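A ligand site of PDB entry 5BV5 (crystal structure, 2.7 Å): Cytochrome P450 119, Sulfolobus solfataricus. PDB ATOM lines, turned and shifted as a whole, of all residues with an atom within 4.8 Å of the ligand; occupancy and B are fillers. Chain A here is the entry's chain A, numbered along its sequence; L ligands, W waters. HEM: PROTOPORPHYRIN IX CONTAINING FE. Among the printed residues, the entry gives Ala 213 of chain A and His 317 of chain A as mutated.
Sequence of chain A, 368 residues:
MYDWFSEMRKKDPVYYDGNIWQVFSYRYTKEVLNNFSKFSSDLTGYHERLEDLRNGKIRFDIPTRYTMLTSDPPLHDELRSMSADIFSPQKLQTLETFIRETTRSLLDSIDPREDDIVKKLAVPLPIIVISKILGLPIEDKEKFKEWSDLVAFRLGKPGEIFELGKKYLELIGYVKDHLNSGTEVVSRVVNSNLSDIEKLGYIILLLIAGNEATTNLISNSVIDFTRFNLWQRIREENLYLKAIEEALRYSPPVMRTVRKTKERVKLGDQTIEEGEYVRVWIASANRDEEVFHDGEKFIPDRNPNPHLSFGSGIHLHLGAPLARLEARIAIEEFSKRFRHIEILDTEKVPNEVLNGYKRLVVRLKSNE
A ring nitrogen (NE2) of His 317 binds an iron atom (FE) of the ligand (1.9 Å).
The backbone NH of Ser 312 lies within hydrogen-bond range of an oxygen (O2A) of the ligand.
The side-chain hydroxyl (OG1) of Thr 257 is in hydrogen-bond range of an oxygen (O1A) of the ligand (3.1 Å).
NH1 of Arg 259 lies within salt-bridge range of O1A of the ligand (3.2 Å).
ND1 of His 317 sits at hydrogen-bond distance from N of Gly 319, at 3.3 Å.
The backbone carbonyl oxygen of Leu 207 sits close to the side-chain amide oxygen of Asn 211.
The side-chain hydroxyl of Ser 309 is in hydrogen-bond range of the backbone carbonyl oxygen of Leu 248 (2.7 Å).
O of Leu 33 lies within hydrogen-bond range of NH2 of Arg 259, at 3.1 Å.
Merely in contact with the ligand: Leu 207 (3.2 Å), Ser 309 (3.2 Å), Gly 210 (3.3 Å), Ala 213 (3.3 Å), Phe 310 (3.6 Å), Val 254 (3.6 Å), Thr 214 (3.6 Å), Asn 211 (3.6 Å), Ala 323 (3.6 Å), Leu 217 (3.7 Å), Gly 311 (3.7 Å), Pro 253 (3.8 Å), Gly 319 (3.8 Å) and Ile 282 (3.999 Å).
Within 4 Å of the ligand: Leu 207, Gly 210, Asn 211, Ala 213, Thr 214, Leu 217, Pro 253, Val 254, Thr 257, Arg 259, Ile 282, Ser 309, Phe 310, Gly 311, Ser 312, His 317, Gly 319 and Ala 323.
The nearest printed residue that does not touch the ligand is Phe 87 (4.05 Å).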
ATOM      1  N   LEU A  33      -7.029  -6.188   9.816  1.00  0.00           N
ATOM      2  CA  LEU A  33      -7.722  -6.582  11.034  1.00  0.00           C
ATOM      3  C   LEU A  33      -9.244  -6.545  10.886  1.00  0.00           C
ATOM      4  O   LEU A  33      -9.944  -7.427  11.385  1.00  0.00           O
ATOM      5  CB  LEU A  33      -7.308  -5.693  12.213  1.00  0.00           C
ATOM      6  CG  LEU A  33      -5.816  -5.670  12.580  1.00  0.00           C
ATOM      7  CD1 LEU A  33      -5.574  -4.671  13.711  1.00  0.00           C
ATOM      8  CD2 LEU A  33      -5.314  -7.048  12.975  1.00  0.00           C
ATOM      9  N   PHE A  87     -18.937  -7.789  31.934  1.00  0.00           N
ATOM     10  CA  PHE A  87     -18.240  -6.520  31.698  1.00  0.00           C
ATOM     11  C   PHE A  87     -19.182  -5.423  31.202  1.00  0.00           C
ATOM     12  O   PHE A  87     -18.792  -4.591  30.380  1.00  0.00           O
ATOM     13  CB  PHE A  87     -17.087  -6.689  30.706  1.00  0.00           C
ATOM     14  CG  PHE A  87     -16.098  -7.757  31.085  1.00  0.00           C
ATOM     15  CD1 PHE A  87     -15.579  -7.818  32.365  1.00  0.00           C
ATOM     16  CD2 PHE A  87     -15.680  -8.685  30.139  1.00  0.00           C
ATOM     17  CE1 PHE A  87     -14.657  -8.793  32.703  1.00  0.00           C
ATOM     18  CE2 PHE A  87     -14.755  -9.668  30.476  1.00  0.00           C
ATOM     19  CZ  PHE A  87     -14.245  -9.723  31.769  1.00  0.00           C
ATOM     20  N   LEU A 206      -9.120 -17.851  29.395  1.00  0.00           N
ATOM     21  CA  LEU A 206      -8.941 -16.648  28.567  1.00  0.00           C
ATOM     22  C   LEU A 206      -9.161 -15.372  29.369  1.00  0.00           C
ATOM     23  O   LEU A 206      -8.349 -14.447  29.303  1.00  0.00           O
ATOM     24  CB  LEU A 206      -9.894 -16.667  27.357  1.00  0.00           C
ATOM     25  CG  LEU A 206      -9.328 -17.165  26.025  1.00  0.00           C
ATOM     26  CD1 LEU A 206      -8.486 -18.418  26.184  1.00  0.00           C
ATOM     27  CD2 LEU A 206     -10.453 -17.375  25.024  1.00  0.00           C
ATOM     28  N   LEU A 207     -10.261 -15.318  30.118  1.00  0.00           N
ATOM     29  CA  LEU A 207     -10.616 -14.142  30.898  1.00  0.00           C
ATOM     30  C   LEU A 207      -9.560 -13.819  31.959  1.00  0.00           C
ATOM     31  O   LEU A 207      -9.340 -12.655  32.290  1.00  0.00           O
ATOM     32  CB  LEU A 207     -11.975 -14.316  31.561  1.00  0.00           C
ATOM     33  CG  LEU A 207     -13.176 -14.427  30.613  1.00  0.00           C
ATOM     34  CD1 LEU A 207     -14.417 -14.890  31.370  1.00  0.00           C
ATOM     35  CD2 LEU A 207     -13.436 -13.096  29.915  1.00  0.00           C
ATOM     36  N   GLY A 210      -5.979 -12.800  29.758  1.00  0.00           N
ATOM     37  CA  GLY A 210      -5.975 -11.472  29.140  1.00  0.00           C
ATOM     38  C   GLY A 210      -5.477 -10.357  30.035  1.00  0.00           C
ATOM     39  O   GLY A 210      -5.043  -9.304  29.548  1.00  0.00           O
ATOM     40  N   ASN A 211      -5.526 -10.578  31.352  1.00  0.00           N
ATOM     41  CA  ASN A 211      -5.130  -9.575  32.332  1.00  0.00           C
ATOM     42  C   ASN A 211      -3.618  -9.295  32.377  1.00  0.00           C
ATOM     43  O   ASN A 211      -3.184  -8.358  33.043  1.00  0.00           O
ATOM     44  CB  ASN A 211      -5.620  -9.974  33.727  1.00  0.00           C
ATOM     45  CG  ASN A 211      -7.139  -9.972  33.829  1.00  0.00           C
ATOM     46  OD1 ASN A 211      -7.746 -11.018  34.048  1.00  0.00           O
ATOM     47  ND2 ASN A 211      -7.743  -8.804  33.669  1.00  0.00           N
ATOM     48  N   ALA A 213      -1.896  -8.300  29.754  1.00  0.00           N
ATOM     49  CA  ALA A 213      -1.756  -7.080  28.965  1.00  0.00           C
ATOM     50  C   ALA A 213      -2.124  -5.846  29.775  1.00  0.00           C
ATOM     51  O   ALA A 213      -1.518  -4.780  29.616  1.00  0.00           O
ATOM     52  CB  ALA A 213      -2.601  -7.166  27.702  1.00  0.00           C
ATOM     53  N   THR A 214      -3.120  -5.991  30.647  1.00  0.00           N
ATOM     54  CA  THR A 214      -3.522  -4.919  31.558  1.00  0.00           C
ATOM     55  C   THR A 214      -2.413  -4.629  32.568  1.00  0.00           C
ATOM     56  O   THR A 214      -2.157  -3.473  32.901  1.00  0.00           O
ATOM     57  CB  THR A 214      -4.801  -5.299  32.329  1.00  0.00           C
ATOM     58  OG1 THR A 214      -5.839  -5.629  31.409  1.00  0.00           O
ATOM     59  CG2 THR A 214      -5.262  -4.142  33.219  1.00  0.00           C
ATOM     60  N   LEU A 217       0.095  -2.679  30.636  1.00  0.00           N
ATOM     61  CA  LEU A 217      -0.360  -1.308  30.406  1.00  0.00           C
ATOM     62  C   LEU A 217      -0.090  -0.417  31.620  1.00  0.00           C
ATOM     63  O   LEU A 217       0.333   0.733  31.469  1.00  0.00           O
ATOM     64  CB  LEU A 217      -1.850  -1.266  30.054  1.00  0.00           C
ATOM     65  CG  LEU A 217      -2.458   0.124  29.849  1.00  0.00           C
ATOM     66  CD1 LEU A 217      -1.684   0.925  28.822  1.00  0.00           C
ATOM     67  CD2 LEU A 217      -3.924   0.005  29.452  1.00  0.00           C
ATOM     68  N   LEU A 248      -1.419   3.461  25.685  1.00  0.00           N
ATOM     69  CA  LEU A 248      -1.834   2.365  24.798  1.00  0.00           C
ATOM     70  C   LEU A 248      -1.275   2.535  23.392  1.00  0.00           C
ATOM     71  O   LEU A 248      -0.739   1.589  22.821  1.00  0.00           O
ATOM     72  CB  LEU A 248      -3.362   2.250  24.746  1.00  0.00           C
ATOM     73  CG  LEU A 248      -4.007   1.439  25.877  1.00  0.00           C
ATOM     74  CD1 LEU A 248      -5.499   1.717  25.953  1.00  0.00           C
ATOM     75  CD2 LEU A 248      -3.747  -0.046  25.678  1.00  0.00           C
ATOM     76  N   PRO A 253       0.715  -2.993  24.854  1.00  0.00           N
ATOM     77  CA  PRO A 253       1.037  -4.291  25.463  1.00  0.00           C
ATOM     78  C   PRO A 253       1.167  -5.436  24.457  1.00  0.00           C
ATOM     79  O   PRO A 253       2.027  -6.302  24.627  1.00  0.00           O
ATOM     80  CB  PRO A 253      -0.159  -4.539  26.390  1.00  0.00           C
ATOM     81  CG  PRO A 253      -0.597  -3.173  26.785  1.00  0.00           C
ATOM     82  CD  PRO A 253      -0.407  -2.331  25.557  1.00  0.00           C
ATOM     83  N   VAL A 254       0.310  -5.456  23.440  1.00  0.00           N
ATOM     84  CA  VAL A 254       0.439  -6.399  22.338  1.00  0.00           C
ATOM     85  C   VAL A 254       1.036  -5.657  21.141  1.00  0.00           C
ATOM     86  O   VAL A 254       0.408  -4.766  20.563  1.00  0.00           O
ATOM     87  CB  VAL A 254      -0.931  -7.015  21.962  1.00  0.00           C
ATOM     88  CG1 VAL A 254      -0.781  -7.992  20.806  1.00  0.00           C
ATOM     89  CG2 VAL A 254      -1.558  -7.693  23.172  1.00  0.00           C
ATOM     90  N   THR A 257       0.048  -8.766  15.798  1.00  0.00           N
ATOM     91  CA  THR A 257      -0.870  -9.895  15.687  1.00  0.00           C
ATOM     92  C   THR A 257      -0.765 -10.480  14.277  1.00  0.00           C
ATOM     93  O   THR A 257      -0.140  -9.883  13.403  1.00  0.00           O
ATOM     94  CB  THR A 257      -2.323  -9.481  16.012  1.00  0.00           C
ATOM     95  OG1 THR A 257      -3.177 -10.631  15.990  1.00  0.00           O
ATOM     96  CG2 THR A 257      -2.828  -8.454  15.013  1.00  0.00           C
ATOM     97  N   ARG A 259      -2.620 -12.592  10.831  1.00  0.00           N
ATOM     98  CA  ARG A 259      -3.796 -12.984  10.051  1.00  0.00           C
ATOM     99  C   ARG A 259      -3.377 -13.908   8.908  1.00  0.00           C
ATOM    100  O   ARG A 259      -2.227 -13.875   8.460  1.00  0.00           O
ATOM    101  CB  ARG A 259      -4.489 -11.755   9.475  1.00  0.00           C
ATOM    102  CG  ARG A 259      -5.243 -10.926  10.510  1.00  0.00           C
ATOM    103  CD  ARG A 259      -6.510 -11.616  10.990  1.00  0.00           C
ATOM    104  NE  ARG A 259      -7.448 -10.664  11.587  1.00  0.00           N
ATOM    105  CZ  ARG A 259      -7.360 -10.167  12.821  1.00  0.00           C
ATOM    106  NH1 ARG A 259      -6.374 -10.533  13.637  1.00  0.00           N
ATOM    107  NH2 ARG A 259      -8.278  -9.300  13.253  1.00  0.00           N
ATOM    108  N   ILE A 282       1.063  -3.663  15.087  1.00  0.00           N
ATOM    109  CA  ILE A 282       0.185  -2.691  15.730  1.00  0.00           C
ATOM    110  C   ILE A 282       1.017  -1.525  16.262  1.00  0.00           C
ATOM    111  O   ILE A 282       0.617  -0.359  16.125  1.00  0.00           O
ATOM    112  CB  ILE A 282      -0.607  -3.352  16.876  1.00  0.00           C
ATOM    113  CG1 ILE A 282      -1.663  -4.298  16.290  1.00  0.00           C
ATOM    114  CG2 ILE A 282      -1.275  -2.299  17.751  1.00  0.00           C
ATOM    115  CD1 ILE A 282      -2.165  -5.352  17.259  1.00  0.00           C
ATOM    116  N   SER A 309      -4.354  -0.711  19.342  1.00  0.00           N
ATOM    117  CA  SER A 309      -3.765  -1.539  20.389  1.00  0.00           C
ATOM    118  C   SER A 309      -4.654  -2.710  20.821  1.00  0.00           C
ATOM    119  O   SER A 309      -4.142  -3.746  21.262  1.00  0.00           O
ATOM    120  CB  SER A 309      -3.416  -0.684  21.607  1.00  0.00           C
ATOM    121  OG  SER A 309      -2.489   0.329  21.271  1.00  0.00           O
ATOM    122  N   PHE A 310      -5.969  -2.558  20.697  1.00  0.00           N
ATOM    123  CA  PHE A 310      -6.911  -3.629  21.021  1.00  0.00           C
ATOM    124  C   PHE A 310      -7.255  -4.493  19.813  1.00  0.00           C
ATOM    125  O   PHE A 310      -7.987  -5.475  19.935  1.00  0.00           O
ATOM    126  CB  PHE A 310      -8.180  -3.049  21.642  1.00  0.00           C
ATOM    127  CG  PHE A 310      -8.004  -2.598  23.063  1.00  0.00           C
ATOM    128  CD1 PHE A 310      -7.888  -3.530  24.089  1.00  0.00           C
ATOM    129  CD2 PHE A 310      -7.944  -1.246  23.379  1.00  0.00           C
ATOM    130  CE1 PHE A 310      -7.715  -3.121  25.401  1.00  0.00           C
ATOM    131  CE2 PHE A 310      -7.780  -0.840  24.694  1.00  0.00           C
ATOM    132  CZ  PHE A 310      -7.657  -1.769  25.707  1.00  0.00           C
ATOM    133  N   GLY A 311      -6.721  -4.135  18.647  1.00  0.00           N
ATOM    134  CA  GLY A 311      -6.852  -4.945  17.445  1.00  0.00           C
ATOM    135  C   GLY A 311      -8.097  -4.607  16.643  1.00  0.00           C
ATOM    136  O   GLY A 311      -8.376  -3.429  16.403  1.00  0.00           O
ATOM    137  N   SER A 312      -8.840  -5.638  16.255  1.00  0.00           N
ATOM    138  CA  SER A 312     -10.002  -5.503  15.373  1.00  0.00           C
ATOM    139  C   SER A 312     -10.885  -4.304  15.723  1.00  0.00           C
ATOM    140  O   SER A 312     -11.751  -4.382  16.600  1.00  0.00           O
ATOM    141  CB  SER A 312     -10.824  -6.791  15.404  1.00  0.00           C
ATOM    142  OG  SER A 312     -11.959  -6.711  14.551  1.00  0.00           O
ATOM    143  N   HIS A 317     -12.970  -5.192  21.223  1.00  0.00           N
ATOM    144  CA  HIS A 317     -12.286  -6.049  22.178  1.00  0.00           C
ATOM    145  C   HIS A 317     -13.081  -6.088  23.488  1.00  0.00           C
ATOM    146  O   HIS A 317     -13.490  -5.054  24.002  1.00  0.00           O
ATOM    147  CB  HIS A 317     -10.856  -5.536  22.392  1.00  0.00           C
ATOM    148  CG  HIS A 317     -10.033  -6.386  23.302  1.00  0.00           C
ATOM    149  ND1 HIS A 317     -10.220  -6.402  24.669  1.00  0.00           N
ATOM    150  CD2 HIS A 317      -8.981  -7.208  23.061  1.00  0.00           C
ATOM    151  CE1 HIS A 317      -9.341  -7.215  25.222  1.00  0.00           C
ATOM    152  NE2 HIS A 317      -8.582  -7.725  24.268  1.00  0.00           N
ATOM    153  N   LEU A 318     -13.274  -7.301  24.010  1.00  0.00           N
ATOM    154  CA  LEU A 318     -14.231  -7.552  25.086  1.00  0.00           C
ATOM    155  C   LEU A 318     -13.828  -6.988  26.445  1.00  0.00           C
ATOM    156  O   LEU A 318     -14.642  -6.376  27.128  1.00  0.00           O
ATOM    157  CB  LEU A 318     -14.476  -9.063  25.219  1.00  0.00           C
ATOM    158  N   GLY A 319     -12.580  -7.211  26.837  1.00  0.00           N
ATOM    159  CA  GLY A 319     -12.075  -6.737  28.126  1.00  0.00           C
ATOM    160  C   GLY A 319     -11.400  -5.374  28.095  1.00  0.00           C
ATOM    161  O   GLY A 319     -10.645  -5.049  29.013  1.00  0.00           O
ATOM    162  N   LEU A 322     -12.742  -3.001  30.838  1.00  0.00           N
ATOM    163  CA  LEU A 322     -12.202  -3.490  32.112  1.00  0.00           C
ATOM    164  C   LEU A 322     -10.745  -3.084  32.286  1.00  0.00           C
ATOM    165  O   LEU A 322     -10.353  -2.592  33.343  1.00  0.00           O
ATOM    166  CB  LEU A 322     -12.306  -5.013  32.180  1.00  0.00           C
ATOM    167  CG  LEU A 322     -11.748  -5.687  33.441  1.00  0.00           C
ATOM    168  CD1 LEU A 322     -12.697  -5.492  34.619  1.00  0.00           C
ATOM    169  CD2 LEU A 322     -11.476  -7.156  33.187  1.00  0.00           C
ATOM    170  N   ALA A 323      -9.941  -3.322  31.250  1.00  0.00           N
ATOM    171  CA  ALA A 323      -8.529  -2.971  31.263  1.00  0.00           C
ATOM    172  C   ALA A 323      -8.349  -1.480  31.519  1.00  0.00           C
ATOM    173  O   ALA A 323      -7.555  -1.076  32.361  1.00  0.00           O
ATOM    174  CB  ALA A 323      -7.859  -3.369  29.962  1.00  0.00           C
HETATM  175  CHA HEM L   1      -7.277 -10.436  21.876  1.00  0.00           C
HETATM  176  CHB HEM L   1      -4.938  -6.462  23.365  1.00  0.00           C
HETATM  177  CHC HEM L   1      -6.803  -7.031  27.820  1.00  0.00           C
HETATM  178  CHD HEM L   1      -9.157 -10.978  26.312  1.00  0.00           C
HETATM  179  C1A HEM L   1      -6.486  -9.318  21.906  1.00  0.00           C
HETATM  180  C2A HEM L   1      -5.789  -8.787  20.802  1.00  0.00           C
HETATM  181  C3A HEM L   1      -5.138  -7.673  21.207  1.00  0.00           C
HETATM  182  C4A HEM L   1      -5.418  -7.510  22.584  1.00  0.00           C
HETATM  183  CMA HEM L   1      -4.275  -6.790  20.337  1.00  0.00           C
HETATM  184  CAA HEM L   1      -5.791  -9.346  19.397  1.00  0.00           C
HETATM  185  CBA HEM L   1      -7.075  -8.886  18.698  1.00  0.00           C
HETATM  186  CGA HEM L   1      -6.944  -9.026  17.201  1.00  0.00           C
HETATM  187  O1A HEM L   1      -6.049  -9.729  16.700  1.00  0.00           O
HETATM  188  O2A HEM L   1      -7.755  -8.419  16.459  1.00  0.00           O
HETATM  189  C1B HEM L   1      -5.256  -6.281  24.709  1.00  0.00           C
HETATM  190  C2B HEM L   1      -4.734  -5.219  25.499  1.00  0.00           C
HETATM  191  C3B HEM L   1      -5.248  -5.349  26.758  1.00  0.00           C
HETATM  192  C4B HEM L   1      -6.111  -6.555  26.711  1.00  0.00           C
HETATM  193  CMB HEM L   1      -3.795  -4.146  25.001  1.00  0.00           C
HETATM  194  CAB HEM L   1      -5.046  -4.514  27.972  1.00  0.00           C
HETATM  195  CBB HEM L   1      -4.330  -3.391  28.019  1.00  0.00           C
HETATM  196  C1C HEM L   1      -7.619  -8.158  27.807  1.00  0.00           C
HETATM  197  C2C HEM L   1      -8.413  -8.596  28.877  1.00  0.00           C
HETATM  198  C3C HEM L   1      -9.094  -9.731  28.460  1.00  0.00           C
HETATM  199  C4C HEM L   1      -8.701  -9.971  27.112  1.00  0.00           C
HETATM  200  CMC HEM L   1      -8.488  -7.925  30.231  1.00  0.00           C
HETATM  201  CAC HEM L   1     -10.070 -10.587  29.190  1.00  0.00           C
HETATM  202  CBC HEM L   1     -10.474 -10.360  30.439  1.00  0.00           C
HETATM  203  C1D HEM L   1      -8.796 -11.091  24.974  1.00  0.00           C
HETATM  204  C2D HEM L   1      -9.322 -12.208  24.178  1.00  0.00           C
HETATM  205  C3D HEM L   1      -8.804 -12.066  22.948  1.00  0.00           C
HETATM  206  C4D HEM L   1      -7.963 -10.857  23.001  1.00  0.00           C
HETATM  207  CMD HEM L   1     -10.247 -13.307  24.654  1.00  0.00           C
HETATM  208  CAD HEM L   1      -9.054 -12.983  21.772  1.00  0.00           C
HETATM  209  CBD HEM L   1     -10.510 -12.884  21.295  1.00  0.00           C
HETATM  210  CGD HEM L   1     -10.915 -11.452  21.007  1.00  0.00           C
HETATM  211  O1D HEM L   1     -10.168 -10.710  20.330  1.00  0.00           O
HETATM  212  O2D HEM L   1     -12.020 -11.023  21.422  1.00  0.00           O
HETATM  213  NA  HEM L   1      -6.221  -8.533  23.005  1.00  0.00           N
HETATM  214  NB  HEM L   1      -6.061  -7.046  25.463  1.00  0.00           N
HETATM  215  NC  HEM L   1      -7.785  -9.014  26.741  1.00  0.00           N
HETATM  216  ND  HEM L   1      -7.984 -10.303  24.237  1.00  0.00           N
HETATM  217 FE   HEM L   1      -7.096  -8.736  24.779  1.00  0.00          FE
HETATM  218  O   HOH W   1      -5.408  -9.750  25.304  1.00  0.00           O
